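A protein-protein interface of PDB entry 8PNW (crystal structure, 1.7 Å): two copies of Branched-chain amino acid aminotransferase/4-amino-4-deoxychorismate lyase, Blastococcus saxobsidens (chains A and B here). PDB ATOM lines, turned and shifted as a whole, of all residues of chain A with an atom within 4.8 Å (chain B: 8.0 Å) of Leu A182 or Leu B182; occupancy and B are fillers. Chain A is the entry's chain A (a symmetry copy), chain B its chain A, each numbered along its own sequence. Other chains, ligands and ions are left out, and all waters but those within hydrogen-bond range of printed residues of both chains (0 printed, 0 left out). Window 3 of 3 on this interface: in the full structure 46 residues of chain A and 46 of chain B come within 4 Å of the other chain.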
ATOM      1  N   GLY A 138     -14.452   7.074  -7.099  1.00  0.00           N
ATOM      2  CA  GLY A 138     -13.205   7.384  -7.815  1.00  0.00           C
ATOM      3  C   GLY A 138     -13.459   8.294  -9.004  1.00  0.00           C
ATOM      4  O   GLY A 138     -12.508   8.628  -9.716  1.00  0.00           O
ATOM      5  N   VAL A 139     -14.689   8.750  -9.223  1.00  0.00           N
ATOM      6  CA  VAL A 139     -14.940   9.592 -10.431  1.00  0.00           C
ATOM      7  C   VAL A 139     -15.128  11.035 -10.006  1.00  0.00           C
ATOM      8  O   VAL A 139     -15.742  11.287  -8.976  1.00  0.00           O
ATOM      9  CB  VAL A 139     -16.135   9.092 -11.238  1.00  0.00           C
ATOM     10  CG1 VAL A 139     -15.812   7.728 -11.821  1.00  0.00           C
ATOM     11  CG2 VAL A 139     -17.394   9.091 -10.400  1.00  0.00           C
ATOM     12  N   PRO A 140     -14.584  12.015 -10.747  1.00  0.00           N
ATOM     13  CA  PRO A 140     -14.917  13.415 -10.477  1.00  0.00           C
ATOM     14  C   PRO A 140     -16.425  13.647 -10.592  1.00  0.00           C
ATOM     15  O   PRO A 140     -17.102  13.034 -11.438  1.00  0.00           O
ATOM     16  CB  PRO A 140     -14.144  14.216 -11.515  1.00  0.00           C
ATOM     17  CG  PRO A 140     -13.120  13.265 -12.053  1.00  0.00           C
ATOM     18  CD  PRO A 140     -13.660  11.866 -11.885  1.00  0.00           C
ATOM     19  N   PHE A 143     -17.668  14.407 -14.162  1.00  0.00           N
ATOM     20  CA  PHE A 143     -17.124  13.564 -15.258  1.00  0.00           C
ATOM     21  C   PHE A 143     -18.250  12.880 -16.048  1.00  0.00           C
ATOM     22  O   PHE A 143     -18.162  12.846 -17.286  1.00  0.00           O
ATOM     23  CB  PHE A 143     -16.094  12.544 -14.731  1.00  0.00           C
ATOM     24  CG  PHE A 143     -15.387  11.814 -15.845  1.00  0.00           C
ATOM     25  CD1 PHE A 143     -14.246  12.349 -16.426  1.00  0.00           C
ATOM     26  CD2 PHE A 143     -15.916  10.642 -16.369  1.00  0.00           C
ATOM     27  CE1 PHE A 143     -13.607  11.699 -17.475  1.00  0.00           C
ATOM     28  CE2 PHE A 143     -15.303  10.027 -17.451  1.00  0.00           C
ATOM     29  CZ  PHE A 143     -14.167  10.572 -18.005  1.00  0.00           C
ATOM     30  N   THR A 180     -19.113   8.734  -2.698  1.00  0.00           N
ATOM     31  CA  THR A 180     -18.508  10.076  -2.845  1.00  0.00           C
ATOM     32  C   THR A 180     -17.675  10.171  -4.127  1.00  0.00           C
ATOM     33  O   THR A 180     -17.114   9.160  -4.589  1.00  0.00           O
ATOM     34  CB  THR A 180     -17.654  10.491  -1.652  1.00  0.00           C
ATOM     35  OG1 THR A 180     -16.523   9.622  -1.533  1.00  0.00           O
ATOM     36  CG2 THR A 180     -18.454  10.503  -0.370  1.00  0.00           C
ATOM     37  N   SER A 181     -17.662  11.366  -4.697  1.00  0.00           N
ATOM     38  CA  SER A 181     -16.858  11.707  -5.896  1.00  0.00           C
ATOM     39  C   SER A 181     -15.392  11.811  -5.478  1.00  0.00           C
ATOM     40  O   SER A 181     -15.086  11.836  -4.279  1.00  0.00           O
ATOM     41  CB  SER A 181     -17.324  13.004  -6.495  1.00  0.00           C
ATOM     42  OG  SER A 181     -16.925  14.093  -5.658  1.00  0.00           O
ATOM     43  N   LEU A 182     -14.489  11.951  -6.445  1.00  0.00           N
ATOM     44  CA  LEU A 182     -13.042  11.974  -6.171  1.00  0.00           C
ATOM     45  C   LEU A 182     -12.708  13.130  -5.206  1.00  0.00           C
ATOM     46  O   LEU A 182     -11.842  12.902  -4.353  1.00  0.00           O
ATOM     47  CB  LEU A 182     -12.351  12.084  -7.535  1.00  0.00           C
ATOM     48  CG  LEU A 182     -10.865  11.796  -7.565  1.00  0.00           C
ATOM     49  CD1 LEU A 182     -10.576  10.403  -7.014  1.00  0.00           C
ATOM     50  CD2 LEU A 182     -10.354  11.952  -8.996  1.00  0.00           C
ATOM     51  N   GLU A 183     -13.388  14.275  -5.348  1.00  0.00           N
ATOM     52  CA  GLU A 183     -13.275  15.556  -4.597  1.00  0.00           C
ATOM     53  C   GLU A 183     -13.922  15.451  -3.215  1.00  0.00           C
ATOM     54  O   GLU A 183     -13.730  16.386  -2.401  1.00  0.00           O
ATOM     55  CB  GLU A 183     -14.088  16.699  -5.240  1.00  0.00           C
ATOM     56  CG  GLU A 183     -13.718  17.060  -6.655  1.00  0.00           C
ATOM     57  CD  GLU A 183     -14.450  16.319  -7.767  1.00  0.00           C
ATOM     58  OE1 GLU A 183     -15.262  15.462  -7.474  1.00  0.00           O
ATOM     59  OE2 GLU A 183     -14.112  16.567  -8.926  1.00  0.00           O
ATOM     60  N   GLY A 184     -14.729  14.422  -2.960  1.00  0.00           N
ATOM     61  CA  GLY A 184     -15.412  14.256  -1.665  1.00  0.00           C
ATOM     62  C   GLY A 184     -16.875  14.666  -1.726  1.00  0.00           C
ATOM     63  O   GLY A 184     -17.495  14.752  -0.669  1.00  0.00           O
ATOM     64  N   GLY B 136     -12.670   7.669 -21.889  1.00  0.00           N
ATOM     65  CA  GLY B 136     -12.211   7.738 -20.479  1.00  0.00           C
ATOM     66  C   GLY B 136     -13.157   6.992 -19.561  1.00  0.00           C
ATOM     67  O   GLY B 136     -14.388   7.098 -19.704  1.00  0.00           O
ATOM     68  N   LEU B 137     -12.606   6.285 -18.595  1.00  0.00           N
ATOM     69  CA  LEU B 137     -13.360   5.607 -17.512  1.00  0.00           C
ATOM     70  C   LEU B 137     -13.643   6.570 -16.346  1.00  0.00           C
ATOM     71  O   LEU B 137     -14.533   6.268 -15.528  1.00  0.00           O
ATOM     72  CB  LEU B 137     -12.479   4.441 -17.069  1.00  0.00           C
ATOM     73  CG  LEU B 137     -13.197   3.178 -16.664  1.00  0.00           C
ATOM     74  CD1 LEU B 137     -14.190   2.759 -17.746  1.00  0.00           C
ATOM     75  CD2 LEU B 137     -12.171   2.102 -16.380  1.00  0.00           C
ATOM     76  N   GLY B 138     -12.882   7.661 -16.254  1.00  0.00           N
ATOM     77  CA  GLY B 138     -13.048   8.736 -15.264  1.00  0.00           C
ATOM     78  C   GLY B 138     -12.343   8.404 -13.961  1.00  0.00           C
ATOM     79  O   GLY B 138     -12.407   9.205 -13.024  1.00  0.00           O
ATOM     80  N   VAL B 139     -11.632   7.283 -13.873  1.00  0.00           N
ATOM     81  CA  VAL B 139     -10.996   6.935 -12.567  1.00  0.00           C
ATOM     82  C   VAL B 139      -9.500   7.166 -12.661  1.00  0.00           C
ATOM     83  O   VAL B 139      -8.909   6.886 -13.696  1.00  0.00           O
ATOM     84  CB  VAL B 139     -11.309   5.503 -12.143  1.00  0.00           C
ATOM     85  CG1 VAL B 139     -12.795   5.378 -11.854  1.00  0.00           C
ATOM     86  CG2 VAL B 139     -10.825   4.512 -13.178  1.00  0.00           C
ATOM     87  N   PRO B 140      -8.852   7.712 -11.618  1.00  0.00           N
ATOM     88  CA  PRO B 140      -7.390   7.759 -11.601  1.00  0.00           C
ATOM     89  C   PRO B 140      -6.798   6.353 -11.719  1.00  0.00           C
ATOM     90  O   PRO B 140      -7.361   5.378 -11.187  1.00  0.00           O
ATOM     91  CB  PRO B 140      -7.027   8.413 -10.276  1.00  0.00           C
ATOM     92  CG  PRO B 140      -8.295   9.051  -9.799  1.00  0.00           C
ATOM     93  CD  PRO B 140      -9.448   8.282 -10.397  1.00  0.00           C
ATOM     94  N   ALA B 141      -5.647   6.275 -12.373  1.00  0.00           N
ATOM     95  CA  ALA B 141      -4.939   5.003 -12.580  1.00  0.00           C
ATOM     96  C   ALA B 141      -4.740   4.318 -11.223  1.00  0.00           C
ATOM     97  O   ALA B 141      -4.849   3.098 -11.152  1.00  0.00           O
ATOM     98  CB  ALA B 141      -3.610   5.246 -13.269  1.00  0.00           C
ATOM     99  N   ASP B 142      -4.421   5.066 -10.179  1.00  0.00           N
ATOM    100  CA  ASP B 142      -3.999   4.455  -8.887  1.00  0.00           C
ATOM    101  C   ASP B 142      -5.197   4.186  -7.965  1.00  0.00           C
ATOM    102  O   ASP B 142      -4.991   3.728  -6.846  1.00  0.00           O
ATOM    103  CB  ASP B 142      -3.010   5.371  -8.169  1.00  0.00           C
ATOM    104  CG  ASP B 142      -1.638   5.425  -8.822  1.00  0.00           C
ATOM    105  OD1 ASP B 142      -1.351   4.512  -9.618  1.00  0.00           O
ATOM    106  OD2 ASP B 142      -0.873   6.350  -8.493  1.00  0.00           O
ATOM    107  N   PHE B 143      -6.424   4.481  -8.369  1.00  0.00           N
ATOM    108  CA  PHE B 143      -7.570   4.553  -7.426  1.00  0.00           C
ATOM    109  C   PHE B 143      -8.073   3.151  -7.048  1.00  0.00           C
ATOM    110  O   PHE B 143      -8.360   2.930  -5.861  1.00  0.00           O
ATOM    111  CB  PHE B 143      -8.706   5.438  -7.979  1.00  0.00           C
ATOM    112  CG  PHE B 143      -9.790   5.685  -6.961  1.00  0.00           C
ATOM    113  CD1 PHE B 143      -9.689   6.740  -6.065  1.00  0.00           C
ATOM    114  CD2 PHE B 143     -10.860   4.808  -6.842  1.00  0.00           C
ATOM    115  CE1 PHE B 143     -10.668   6.955  -5.102  1.00  0.00           C
ATOM    116  CE2 PHE B 143     -11.805   4.998  -5.844  1.00  0.00           C
ATOM    117  CZ  PHE B 143     -11.688   6.057  -4.973  1.00  0.00           C
ATOM    118  N   PHE B 179     -10.076   1.853 -23.040  1.00  0.00           N
ATOM    119  CA  PHE B 179     -10.358   2.740 -21.895  1.00  0.00           C
ATOM    120  C   PHE B 179      -9.088   3.425 -21.428  1.00  0.00           C
ATOM    121  O   PHE B 179      -7.984   2.780 -21.385  1.00  0.00           O
ATOM    122  CB  PHE B 179     -10.982   2.005 -20.718  1.00  0.00           C
ATOM    123  CG  PHE B 179     -12.423   1.600 -20.943  1.00  0.00           C
ATOM    124  CD1 PHE B 179     -13.390   2.553 -21.233  1.00  0.00           C
ATOM    125  CD2 PHE B 179     -12.815   0.277 -20.824  1.00  0.00           C
ATOM    126  CE1 PHE B 179     -14.709   2.179 -21.429  1.00  0.00           C
ATOM    127  CE2 PHE B 179     -14.150  -0.084 -20.961  1.00  0.00           C
ATOM    128  CZ  PHE B 179     -15.091   0.875 -21.279  1.00  0.00           C
ATOM    129  N   THR B 180      -9.272   4.656 -20.921  1.00  0.00           N
ATOM    130  CA  THR B 180      -8.186   5.480 -20.346  1.00  0.00           C
ATOM    131  C   THR B 180      -8.553   5.980 -18.946  1.00  0.00           C
ATOM    132  O   THR B 180      -9.744   6.186 -18.643  1.00  0.00           O
ATOM    133  CB  THR B 180      -7.792   6.663 -21.222  1.00  0.00           C
ATOM    134  OG1 THR B 180      -8.887   7.578 -21.332  1.00  0.00           O
ATOM    135  CG2 THR B 180      -7.331   6.216 -22.590  1.00  0.00           C
ATOM    136  N   SER B 181      -7.532   6.111 -18.113  1.00  0.00           N
ATOM    137  CA  SER B 181      -7.643   6.657 -16.738  1.00  0.00           C
ATOM    138  C   SER B 181      -7.848   8.168 -16.837  1.00  0.00           C
ATOM    139  O   SER B 181      -7.679   8.751 -17.915  1.00  0.00           O
ATOM    140  CB  SER B 181      -6.406   6.348 -15.944  1.00  0.00           C
ATOM    141  OG  SER B 181      -5.321   7.159 -16.405  1.00  0.00           O
ATOM    142  N   LEU B 182      -8.132   8.821 -15.713  1.00  0.00           N
ATOM    143  CA  LEU B 182      -8.435  10.262 -15.698  1.00  0.00           C
ATOM    144  C   LEU B 182      -7.246  11.056 -16.276  1.00  0.00           C
ATOM    145  O   LEU B 182      -7.528  12.033 -16.981  1.00  0.00           O
ATOM    146  CB  LEU B 182      -8.767  10.612 -14.242  1.00  0.00           C
ATOM    147  CG  LEU B 182      -9.432  11.951 -14.005  1.00  0.00           C
ATOM    148  CD1 LEU B 182     -10.723  12.061 -14.809  1.00  0.00           C
ATOM    149  CD2 LEU B 182      -9.685  12.125 -12.508  1.00  0.00           C
ATOM    150  N   GLU B 183      -6.011  10.622 -15.994  1.00  0.00           N
ATOM    151  CA  GLU B 183      -4.687  11.181 -16.380  1.00  0.00           C
ATOM    152  C   GLU B 183      -4.359  10.878 -17.843  1.00  0.00           C
ATOM    153  O   GLU B 183      -3.371  11.455 -18.358  1.00  0.00           O
ATOM    154  CB  GLU B 183      -3.513  10.501 -15.646  1.00  0.00           C
ATOM    155  CG  GLU B 183      -3.533  10.588 -14.142  1.00  0.00           C
ATOM    156  CD  GLU B 183      -4.253   9.470 -13.398  1.00  0.00           C
ATOM    157  OE1 GLU B 183      -4.798   8.589 -14.035  1.00  0.00           O
ATOM    158  OE2 GLU B 183      -4.323   9.565 -12.171  1.00  0.00           O
ATOM    159  N   GLY B 184      -5.075   9.956 -18.484  1.00  0.00           N
ATOM    160  CA  GLY B 184      -4.812   9.585 -19.886  1.00  0.00           C
ATOM    161  C   GLY B 184      -4.055   8.272 -20.003  1.00  0.00           C
ATOM    162  O   GLY B 184      -3.613   7.957 -21.106  1.00  0.00           O
ATOM    163  N   ARG B 185      -3.884   7.512 -18.913  1.00  0.00           N
ATOM    164  CA  ARG B 185      -3.104   6.256 -18.999  1.00  0.00           C
ATOM    165  C   ARG B 185      -4.006   5.230 -19.690  1.00  0.00           C
ATOM    166  O   ARG B 185      -5.213   5.171 -19.417  1.00  0.00           O
ATOM    167  CB  ARG B 185      -2.595   5.798 -17.626  1.00  0.00           C
ATOM    168  CG  ARG B 185      -1.781   6.829 -16.847  1.00  0.00           C
ATOM    169  CD  ARG B 185      -0.439   6.361 -16.305  1.00  0.00           C
ATOM    170  NE  ARG B 185      -0.262   5.521 -15.084  1.00  0.00           N
ATOM    171  CZ  ARG B 185      -0.267   4.165 -15.016  1.00  0.00           C
ATOM    172  NH1 ARG B 185      -0.575   3.412 -16.070  1.00  0.00           N
ATOM    173  NH2 ARG B 185       0.046   3.546 -13.877  1.00  0.00           N
ATOM    174  N   LEU B 187      -5.733   1.791 -20.029  1.00  0.00           N
ATOM    175  CA  LEU B 187      -6.166   0.708 -19.128  1.00  0.00           C
ATOM    176  C   LEU B 187      -6.278  -0.573 -19.972  1.00  0.00           C
ATOM    177  O   LEU B 187      -5.318  -1.377 -19.999  1.00  0.00           O
ATOM    178  CB  LEU B 187      -7.465   1.168 -18.471  1.00  0.00           C
ATOM    179  CG  LEU B 187      -7.288   2.391 -17.560  1.00  0.00           C
ATOM    180  CD1 LEU B 187      -8.637   2.896 -17.082  1.00  0.00           C
ATOM    181  CD2 LEU B 187      -6.387   2.036 -16.376  1.00  0.00           C
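O of Gly A138 sits close to O of Gly B138 (3.4 Å).
N of Leu B137 sits at hydrogen-bond distance from O of Thr B180, at 2.9 Å.
The backbone carbonyl oxygen (O) of Val B139 lies within hydrogen-bond range of the backbone NH (N) of Leu B182 (2.9 Å).
The backbone carbonyl oxygen (O) of Val A139 sits at hydrogen-bond distance from the backbone NH (N) of Leu A182, at 2.9 Å.
Gly A138 touches Val B139.
O of Gly A138 touches CD of Pro B140, at 3.2 Å.
CE2 of Phe B143 touches CA of Gly A138 (3.4 Å).
Val A139 touches Gly B138 (CA to O, 3.6 Å).
Val A139 touches Val B139 (CG1 to CG1, 3.8 Å).
O of Gly B138 touches CD of Pro A140, at 3.2 Å.
Phe A143 touches Leu B137 (CE2 to C, 3.99 Å).
Leu B182 touches Phe A143.
Leu A182 touches Pro B140.
CD1 of Phe B143 touches CD1 of Leu A182, 3.9 Å away.
Of chain B, only Pro B140 (3.6 Å), Phe B143 (3.9 Å) and Leu B182 (3.6 Å) come within 4 Å of Leu A182.
Ser A181 touches none of the printed residues of chain B.
Of the printed residues of chain B, Val A139 touches Gly B138 and Val B139.
Printed residues of chain A within 4 Å of Gly B138: Gly A138 (3.4 Å), Val A139 (3.6 Å), Pro A140 (3.2 Å) and Phe A143 (3.4 Å).
Of the printed residues of chain A, Pro B140 touches Gly A138 (3.2 Å) and Leu A182 (3.6 Å).
Printed residues of chain A within 4 Å of Val B139: Gly A138 (3.6 Å) and Val A139 (3.8 Å).
Of the printed residues of chain B, Phe A143 touches Gly B136, Leu B137, Gly B138 and Leu B182.
Asp B142 touches none of the printed residues of chain A.
Glu B183 touches none of the printed residues of chain A.
The nearest printed residue of chain A that does not touch Leu B182 is Gly A138 (5.3 Å).
The nearest printed residue of chain B that does not touch Pro A140 is Val B139 (5.4 Å).
Of the 9 printed residues of chain A, 5 touch a printed residue of chain B.
Hydrophobic or aromatic side chains of chain A that line the printed part of chain B: Val A139, Pro A140, Phe A143 and Leu A182.
Printed residues of chain B that touch a printed residue of chain A: Gly B136, Leu B137, Gly B138, Val B139, Pro B140, Phe B143 and Leu B182.
Hydrophobic or aromatic side chains of chain B within 4 Å of the printed part of chain A: Val B139, Pro B140, Phe B143 and Leu B182.
Among the printed residues, 15 pairs touch across the chains.
Gly B138 touches its own counterpart, Gly A138.
Gly A138 touches Val B139, and with the chains exchanged Val A139 touches Gly B138.
Pro A140 touches Leu B182, and with the chains exchanged Leu A182 touches Pro B140.
Leu A182 touches its own counterpart, Leu B182.
Of the 15 pairs that touch across the chains among the printed residues, 13 have their exchanged pair printed and touching as well.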
